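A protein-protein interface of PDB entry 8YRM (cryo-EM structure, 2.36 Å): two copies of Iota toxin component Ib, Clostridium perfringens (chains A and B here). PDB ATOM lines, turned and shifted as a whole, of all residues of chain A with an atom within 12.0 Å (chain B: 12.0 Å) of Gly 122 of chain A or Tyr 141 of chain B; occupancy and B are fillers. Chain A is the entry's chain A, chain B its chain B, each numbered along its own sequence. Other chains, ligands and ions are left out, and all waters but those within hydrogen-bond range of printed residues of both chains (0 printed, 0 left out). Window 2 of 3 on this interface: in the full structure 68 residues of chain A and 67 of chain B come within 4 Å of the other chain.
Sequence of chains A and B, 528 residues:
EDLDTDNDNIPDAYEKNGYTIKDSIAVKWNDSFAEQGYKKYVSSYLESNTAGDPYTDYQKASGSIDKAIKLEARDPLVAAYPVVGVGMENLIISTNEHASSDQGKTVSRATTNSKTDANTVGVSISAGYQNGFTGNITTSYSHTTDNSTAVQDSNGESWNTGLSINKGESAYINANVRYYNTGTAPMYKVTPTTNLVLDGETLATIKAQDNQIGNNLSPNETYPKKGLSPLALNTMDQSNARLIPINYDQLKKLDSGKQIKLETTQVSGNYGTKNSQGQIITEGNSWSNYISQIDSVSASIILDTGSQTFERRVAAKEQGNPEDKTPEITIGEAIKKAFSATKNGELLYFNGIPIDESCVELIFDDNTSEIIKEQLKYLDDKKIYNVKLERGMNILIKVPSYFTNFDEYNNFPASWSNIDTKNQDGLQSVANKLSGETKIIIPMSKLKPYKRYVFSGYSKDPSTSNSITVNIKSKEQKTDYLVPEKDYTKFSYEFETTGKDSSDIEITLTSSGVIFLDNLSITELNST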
ATOM      1  N   ALA A 118      -7.561 -26.670  -1.307  1.00  0.00           N
ATOM      2  CA  ALA A 118      -7.932 -26.180  -2.625  1.00  0.00           C
ATOM      3  C   ALA A 118      -7.597 -27.222  -3.690  1.00  0.00           C
ATOM      4  O   ALA A 118      -6.558 -27.876  -3.621  1.00  0.00           O
ATOM      5  CB  ALA A 118      -7.236 -24.866  -2.904  1.00  0.00           C
ATOM      6  N   ASN A 119      -8.496 -27.355  -4.672  1.00  0.00           N
ATOM      7  CA  ASN A 119      -8.305 -28.245  -5.805  1.00  0.00           C
ATOM      8  C   ASN A 119      -8.556 -27.460  -7.090  1.00  0.00           C
ATOM      9  O   ASN A 119      -9.511 -26.690  -7.165  1.00  0.00           O
ATOM     10  CB  ASN A 119      -9.230 -29.457  -5.734  1.00  0.00           C
ATOM     11  CG  ASN A 119      -9.280 -30.066  -4.353  1.00  0.00           C
ATOM     12  OD1 ASN A 119      -8.300 -30.672  -3.904  1.00  0.00           O
ATOM     13  ND2 ASN A 119     -10.406 -29.928  -3.667  1.00  0.00           N
ATOM     14  N   THR A 120      -7.694 -27.666  -8.093  1.00  0.00           N
ATOM     15  CA  THR A 120      -7.831 -27.007  -9.383  1.00  0.00           C
ATOM     16  C   THR A 120      -7.910 -28.069 -10.477  1.00  0.00           C
ATOM     17  O   THR A 120      -7.090 -28.984 -10.512  1.00  0.00           O
ATOM     18  CB  THR A 120      -6.658 -26.057  -9.626  1.00  0.00           C
ATOM     19  OG1 THR A 120      -6.671 -25.111  -8.562  1.00  0.00           O
ATOM     20  CG2 THR A 120      -6.763 -25.337 -10.959  1.00  0.00           C
ATOM     21  N   VAL A 121      -8.893 -27.915 -11.373  1.00  0.00           N
ATOM     22  CA  VAL A 121      -9.056 -28.787 -12.524  1.00  0.00           C
ATOM     23  C   VAL A 121      -9.045 -27.918 -13.779  1.00  0.00           C
ATOM     24  O   VAL A 121      -9.762 -26.924 -13.848  1.00  0.00           O
ATOM     25  CB  VAL A 121     -10.351 -29.617 -12.429  1.00  0.00           C
ATOM     26  CG1 VAL A 121     -10.550 -30.509 -13.649  1.00  0.00           C
ATOM     27  CG2 VAL A 121     -10.403 -30.449 -11.154  1.00  0.00           C
ATOM     28  N   GLY A 122      -8.228 -28.306 -14.767  1.00  0.00           N
ATOM     29  CA  GLY A 122      -8.114 -27.560 -16.009  1.00  0.00           C
ATOM     30  C   GLY A 122      -7.747 -28.461 -17.175  1.00  0.00           C
ATOM     31  O   GLY A 122      -6.737 -28.148 -17.840  1.00  0.00           O
ATOM     32  N   SER A 140      -5.447 -30.793 -16.761  1.00  0.00           N
ATOM     33  CA  SER A 140      -4.556 -31.089 -15.609  1.00  0.00           C
ATOM     34  C   SER A 140      -5.304 -30.862 -14.298  1.00  0.00           C
ATOM     35  O   SER A 140      -6.217 -30.042 -14.236  1.00  0.00           O
ATOM     36  CB  SER A 140      -3.299 -30.255 -15.669  1.00  0.00           C
ATOM     37  OG  SER A 140      -3.596 -28.869 -15.567  1.00  0.00           O
ATOM     38  N   TYR A 141      -4.894 -31.599 -13.259  1.00  0.00           N
ATOM     39  CA  TYR A 141      -5.477 -31.475 -11.933  1.00  0.00           C
ATOM     40  C   TYR A 141      -4.368 -31.183 -10.926  1.00  0.00           C
ATOM     41  O   TYR A 141      -3.302 -31.792 -10.983  1.00  0.00           O
ATOM     42  CB  TYR A 141      -6.249 -32.746 -11.564  1.00  0.00           C
ATOM     43  CG  TYR A 141      -6.560 -32.868 -10.078  1.00  0.00           C
ATOM     44  CD1 TYR A 141      -7.525 -32.066  -9.480  1.00  0.00           C
ATOM     45  CD2 TYR A 141      -5.890 -33.783  -9.273  1.00  0.00           C
ATOM     46  CE1 TYR A 141      -7.811 -32.167  -8.128  1.00  0.00           C
ATOM     47  CE2 TYR A 141      -6.168 -33.895  -7.920  1.00  0.00           C
ATOM     48  CZ  TYR A 141      -7.132 -33.085  -7.346  1.00  0.00           C
ATOM     49  OH  TYR A 141      -7.414 -33.189  -6.015  1.00  0.00           O
ATOM     50  N   SER A 142      -4.640 -30.249 -10.005  1.00  0.00           N
ATOM     51  CA  SER A 142      -3.692 -29.887  -8.964  1.00  0.00           C
ATOM     52  C   SER A 142      -4.411 -29.811  -7.620  1.00  0.00           C
ATOM     53  O   SER A 142      -5.588 -29.458  -7.558  1.00  0.00           O
ATOM     54  CB  SER A 142      -2.990 -28.587  -9.281  1.00  0.00           C
ATOM     55  OG  SER A 142      -3.732 -27.466  -8.820  1.00  0.00           O
ATOM     56  N   HIS A 143      -3.678 -30.142  -6.551  1.00  0.00           N
ATOM     57  CA  HIS A 143      -4.202 -30.117  -5.195  1.00  0.00           C
ATOM     58  C   HIS A 143      -3.303 -29.229  -4.340  1.00  0.00           C
ATOM     59  O   HIS A 143      -2.083 -29.365  -4.382  1.00  0.00           O
ATOM     60  CB  HIS A 143      -4.274 -31.540  -4.628  1.00  0.00           C
ATOM     61  CG  HIS A 143      -4.838 -31.612  -3.248  1.00  0.00           C
ATOM     62  ND1 HIS A 143      -6.142 -31.982  -3.000  1.00  0.00           N
ATOM     63  CD2 HIS A 143      -4.283 -31.383  -2.050  1.00  0.00           C
ATOM     64  CE1 HIS A 143      -6.359 -31.965  -1.693  1.00  0.00           C
ATOM     65  NE2 HIS A 143      -5.244 -31.602  -1.096  1.00  0.00           N
ATOM     66  N   THR A 144      -3.921 -28.331  -3.563  1.00  0.00           N
ATOM     67  CA  THR A 144      -3.189 -27.404  -2.716  1.00  0.00           C
ATOM     68  C   THR A 144      -3.695 -27.531  -1.282  1.00  0.00           C
ATOM     69  O   THR A 144      -4.901 -27.526  -1.044  1.00  0.00           O
ATOM     70  CB  THR A 144      -3.345 -25.974  -3.234  1.00  0.00           C
ATOM     71  OG1 THR A 144      -3.037 -25.993  -4.625  1.00  0.00           O
ATOM     72  CG2 THR A 144      -2.428 -24.997  -2.520  1.00  0.00           C
ATOM     73  N   LYS B 115     -16.238 -21.378   2.002  1.00  0.00           N
ATOM     74  CA  LYS B 115     -16.212 -22.150   0.769  1.00  0.00           C
ATOM     75  C   LYS B 115     -16.249 -21.178  -0.406  1.00  0.00           C
ATOM     76  O   LYS B 115     -17.117 -20.311  -0.460  1.00  0.00           O
ATOM     77  CB  LYS B 115     -17.412 -23.105   0.751  1.00  0.00           C
ATOM     78  CG  LYS B 115     -17.918 -23.527  -0.626  1.00  0.00           C
ATOM     79  CD  LYS B 115     -17.343 -24.842  -1.136  1.00  0.00           C
ATOM     80  CE  LYS B 115     -17.458 -25.005  -2.621  1.00  0.00           C
ATOM     81  NZ  LYS B 115     -16.498 -24.156  -3.332  1.00  0.00           N
ATOM     82  N   THR B 116     -15.314 -21.341  -1.350  1.00  0.00           N
ATOM     83  CA  THR B 116     -15.225 -20.458  -2.501  1.00  0.00           C
ATOM     84  C   THR B 116     -15.105 -21.285  -3.778  1.00  0.00           C
ATOM     85  O   THR B 116     -14.497 -22.352  -3.783  1.00  0.00           O
ATOM     86  CB  THR B 116     -14.050 -19.492  -2.338  1.00  0.00           C
ATOM     87  OG1 THR B 116     -13.955 -18.759  -3.555  1.00  0.00           O
ATOM     88  CG2 THR B 116     -12.732 -20.199  -2.087  1.00  0.00           C
ATOM     89  N   ASP B 117     -15.700 -20.758  -4.854  1.00  0.00           N
ATOM     90  CA  ASP B 117     -15.696 -21.389  -6.163  1.00  0.00           C
ATOM     91  C   ASP B 117     -15.206 -20.374  -7.190  1.00  0.00           C
ATOM     92  O   ASP B 117     -15.753 -19.278  -7.276  1.00  0.00           O
ATOM     93  CB  ASP B 117     -17.085 -21.891  -6.526  1.00  0.00           C
ATOM     94  CG  ASP B 117     -17.338 -22.069  -8.016  1.00  0.00           C
ATOM     95  OD1 ASP B 117     -18.143 -21.290  -8.570  1.00  0.00           O
ATOM     96  OD2 ASP B 117     -16.721 -22.976  -8.610  1.00  0.00           O
ATOM     97  N   ALA B 118     -14.192 -20.756  -7.975  1.00  0.00           N
ATOM     98  CA  ALA B 118     -13.591 -19.859  -8.949  1.00  0.00           C
ATOM     99  C   ALA B 118     -13.461 -20.554 -10.301  1.00  0.00           C
ATOM    100  O   ALA B 118     -13.128 -21.736 -10.367  1.00  0.00           O
ATOM    101  CB  ALA B 118     -12.246 -19.375  -8.449  1.00  0.00           C
ATOM    102  N   ASN B 119     -13.727 -19.795 -11.371  1.00  0.00           N
ATOM    103  CA  ASN B 119     -13.584 -20.273 -12.737  1.00  0.00           C
ATOM    104  C   ASN B 119     -12.749 -19.265 -13.521  1.00  0.00           C
ATOM    105  O   ASN B 119     -12.955 -18.060 -13.391  1.00  0.00           O
ATOM    106  CB  ASN B 119     -14.938 -20.478 -13.408  1.00  0.00           C
ATOM    107  CG  ASN B 119     -15.930 -21.182 -12.510  1.00  0.00           C
ATOM    108  OD1 ASN B 119     -15.781 -22.378 -12.236  1.00  0.00           O
ATOM    109  ND2 ASN B 119     -16.945 -20.466 -12.049  1.00  0.00           N
ATOM    110  N   THR B 120     -11.812 -19.769 -14.334  1.00  0.00           N
ATOM    111  CA  THR B 120     -10.965 -18.924 -15.161  1.00  0.00           C
ATOM    112  C   THR B 120     -11.122 -19.341 -16.621  1.00  0.00           C
ATOM    113  O   THR B 120     -11.043 -20.525 -16.939  1.00  0.00           O
ATOM    114  CB  THR B 120      -9.507 -19.030 -14.716  1.00  0.00           C
ATOM    115  OG1 THR B 120      -9.464 -18.621 -13.352  1.00  0.00           O
ATOM    116  CG2 THR B 120      -8.581 -18.158 -15.547  1.00  0.00           C
ATOM    117  N   VAL B 121     -11.325 -18.348 -17.495  1.00  0.00           N
ATOM    118  CA  VAL B 121     -11.413 -18.564 -18.931  1.00  0.00           C
ATOM    119  C   VAL B 121     -10.363 -17.686 -19.605  1.00  0.00           C
ATOM    120  O   VAL B 121     -10.279 -16.493 -19.322  1.00  0.00           O
ATOM    121  CB  VAL B 121     -12.827 -18.255 -19.464  1.00  0.00           C
ATOM    122  CG1 VAL B 121     -12.923 -18.444 -20.974  1.00  0.00           C
ATOM    123  CG2 VAL B 121     -13.894 -19.085 -18.762  1.00  0.00           C
ATOM    124  N   GLY B 122      -9.570 -18.287 -20.501  1.00  0.00           N
ATOM    125  CA  GLY B 122      -8.517 -17.568 -21.200  1.00  0.00           C
ATOM    126  C   GLY B 122      -8.241 -18.166 -22.567  1.00  0.00           C
ATOM    127  O   GLY B 122      -7.061 -18.496 -22.817  1.00  0.00           O
ATOM    128  N   SER B 140      -8.111 -21.449 -22.904  1.00  0.00           N
ATOM    129  CA  SER B 140      -8.165 -22.535 -21.891  1.00  0.00           C
ATOM    130  C   SER B 140      -9.149 -22.166 -20.783  1.00  0.00           C
ATOM    131  O   SER B 140      -9.360 -20.987 -20.503  1.00  0.00           O
ATOM    132  CB  SER B 140      -6.795 -22.819 -21.329  1.00  0.00           C
ATOM    133  OG  SER B 140      -6.277 -21.688 -20.639  1.00  0.00           O
ATOM    134  N   TYR B 141      -9.736 -23.194 -20.160  1.00  0.00           N
ATOM    135  CA  TYR B 141     -10.667 -23.014 -19.057  1.00  0.00           C
ATOM    136  C   TYR B 141     -10.177 -23.815 -17.855  1.00  0.00           C
ATOM    137  O   TYR B 141      -9.745 -24.956 -18.004  1.00  0.00           O
ATOM    138  CB  TYR B 141     -12.081 -23.435 -19.473  1.00  0.00           C
ATOM    139  CG  TYR B 141     -13.031 -23.648 -18.302  1.00  0.00           C
ATOM    140  CD1 TYR B 141     -13.526 -22.571 -17.576  1.00  0.00           C
ATOM    141  CD2 TYR B 141     -13.429 -24.924 -17.919  1.00  0.00           C
ATOM    142  CE1 TYR B 141     -14.385 -22.755 -16.506  1.00  0.00           C
ATOM    143  CE2 TYR B 141     -14.290 -25.122 -16.852  1.00  0.00           C
ATOM    144  CZ  TYR B 141     -14.770 -24.034 -16.143  1.00  0.00           C
ATOM    145  OH  TYR B 141     -15.619 -24.221 -15.090  1.00  0.00           O
ATOM    146  N   SER B 142     -10.258 -23.203 -16.667  1.00  0.00           N
ATOM    147  CA  SER B 142      -9.858 -23.853 -15.430  1.00  0.00           C
ATOM    148  C   SER B 142     -10.919 -23.616 -14.358  1.00  0.00           C
ATOM    149  O   SER B 142     -11.572 -22.575 -14.346  1.00  0.00           O
ATOM    150  CB  SER B 142      -8.499 -23.376 -14.969  1.00  0.00           C
ATOM    151  OG  SER B 142      -8.601 -22.204 -14.172  1.00  0.00           O
ATOM    152  N   HIS B 143     -11.066 -24.597 -13.462  1.00  0.00           N
ATOM    153  CA  HIS B 143     -12.024 -24.533 -12.371  1.00  0.00           C
ATOM    154  C   HIS B 143     -11.281 -24.746 -11.055  1.00  0.00           C
ATOM    155  O   HIS B 143     -10.483 -25.673 -10.941  1.00  0.00           O
ATOM    156  CB  HIS B 143     -13.120 -25.587 -12.562  1.00  0.00           C
ATOM    157  CG  HIS B 143     -14.172 -25.568 -11.503  1.00  0.00           C
ATOM    158  ND1 HIS B 143     -15.401 -24.976 -11.692  1.00  0.00           N
ATOM    159  CD2 HIS B 143     -14.189 -26.072 -10.263  1.00  0.00           C
ATOM    160  CE1 HIS B 143     -16.127 -25.119 -10.592  1.00  0.00           C
ATOM    161  NE2 HIS B 143     -15.409 -25.779  -9.710  1.00  0.00           N
ATOM    162  N   THR B 144     -11.560 -23.884 -10.069  1.00  0.00           N
ATOM    163  CA  THR B 144     -10.908 -23.954  -8.771  1.00  0.00           C
ATOM    164  C   THR B 144     -11.974 -24.024  -7.680  1.00  0.00           C
ATOM    165  O   THR B 144     -12.922 -23.242  -7.684  1.00  0.00           O
ATOM    166  CB  THR B 144      -9.991 -22.747  -8.572  1.00  0.00           C
ATOM    167  OG1 THR B 144      -9.165 -22.650  -9.729  1.00  0.00           O
ATOM    168  CG2 THR B 144      -9.123 -22.880  -7.333  1.00  0.00           C
ATOM    169  N   THR B 145     -11.793 -24.970  -6.750  1.00  0.00           N
ATOM    170  CA  THR B 145     -12.644 -25.102  -5.579  1.00  0.00           C
ATOM    171  C   THR B 145     -11.755 -25.129  -4.339  1.00  0.00           C
ATOM    172  O   THR B 145     -10.786 -25.883  -4.293  1.00  0.00           O
ATOM    173  CB  THR B 145     -13.489 -26.370  -5.688  1.00  0.00           C
ATOM    174  OG1 THR B 145     -14.384 -26.156  -6.776  1.00  0.00           O
ATOM    175  CG2 THR B 145     -14.278 -26.658  -4.423  1.00  0.00           C
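Thr 145 of chain B touches Ala 118 of chain A (O to CA, 3.3 Å). Thr 144 of chain B touches Asn 119 of chain A (CA to O, 3.5 Å). CA of Thr 120 of chain A touches O of His 143 of chain B (3.4 Å). Thr 144 of chain B touches Thr 120 of chain A (CG2 to OG1, 3.5 Å). CA of Ser 142 of chain B touches O of Val 121 of chain A (3.5 Å). O of Tyr 141 of chain B touches CA of Gly 122 of chain A, at 3.7 Å.
Thr 120 of chain A touches His 143 of chain B, but with the chains exchanged His 143 of chain A does not touch Thr 120 of chain B (14.6 Å). Val 121 of chain A touches Ser 142 of chain B, but with the chains exchanged Ser 142 of chain A does not touch Val 121 of chain B (14.7 Å). Val 121 of chain A touches His 143 of chain B, but with the chains exchanged His 143 of chain A does not touch Val 121 of chain B (17.8 Å). Gly 122 of chain A touches Tyr 141 of chain B, but with the chains exchanged Tyr 141 of chain A does not touch Gly 122 of chain B (15.9 Å). Positions printed for both chains: 118, 119, 120, 121, 122, 140, 141, 142, 143 and 144. Of the 8 pairs that touch across the chains among the printed residues, none has its exchanged pair printed and touching as well.
Of the 14 printed residues of chain B, 5 touch a printed residue of chain A. Hydrophobic or aromatic side chains of chain A that line the printed part of chain B: Ala 118. Among the printed residues, 8 pairs touch across the chains. Among the printed residues, no Asp or Glu carboxylate lies within 4 Å of a Lys or Arg side-chain nitrogen of the other chain.
Of the printed residues of chain B, Ala 118 of chain A touches Thr 145. Of the printed residues of chain B, Asn 119 of chain A touches Thr 144 (3.5 Å) and Thr 145 (2.7 Å). Thr 120 of chain A touches just these residues of chain B: His 143 (3.4 Å) and Thr 144 (3.5 Å). Gly 122 of chain A touches one residue of chain B. Ser 142 of chain A touches none of the printed residues of chain B. Lys 115 of chain B touches none of the printed residues of chain A. No residue of chain A comes within 4 Å of Asn 119 of chain B. Val 121 of chain B touches none of the printed residues of chain A. No residue of chain A comes within 4 Å of Gly 122 of chain B. Ser 140 of chain B touches none of the printed residues of chain A. Tyr 141 of chain B touches just one residue of chain A: Gly 122 (3.7 Å). Ser 142 of chain B touches one residue of chain A. Of chain A, only Thr 120 (3.4 Å) and Val 121 (2.7 Å) come within 4 Å of His 143 of chain B. Printed residues of chain A within 4 Å of Thr 145 of chain B: Ala 118 and Asn 119.
The backbone carbonyl oxygen (O) of Thr 145 of chain B is in hydrogen-bond range of the backbone NH (N) of Asn 119 of chain A (2.7 Å). The backbone NH (N) of His 143 of chain B sits at hydrogen-bond distance from the backbone carbonyl oxygen (O) of Val 121 of chain A, 2.7 Å away.
The side-chain amide oxygen (OD1) of Asn 119 of chain A is in hydrogen-bond range of the side-chain hydroxyl (OH) of Tyr 141 of chain A (3.4 Å). ND1 of His 143 of chain A lies within hydrogen-bond range of OD1 of Asn 119 of chain A, 2.7 Å away. N of Ser 142 of chain A sits at hydrogen-bond distance from O of Thr 120 of chain A (2.8 Å). NE2 of His 143 of chain B sits close to OD2 of Asp 117 of chain B. A ring nitrogen (ND1) of His 143 of chain B is in hydrogen-bond range of the side-chain amide oxygen of Asn 119 of chain B (2.7 Å). The backbone NH (N) of Ser 142 of chain B is in hydrogen-bond range of the backbone carbonyl oxygen (O) of Thr 120 of chain B (2.8 Å).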
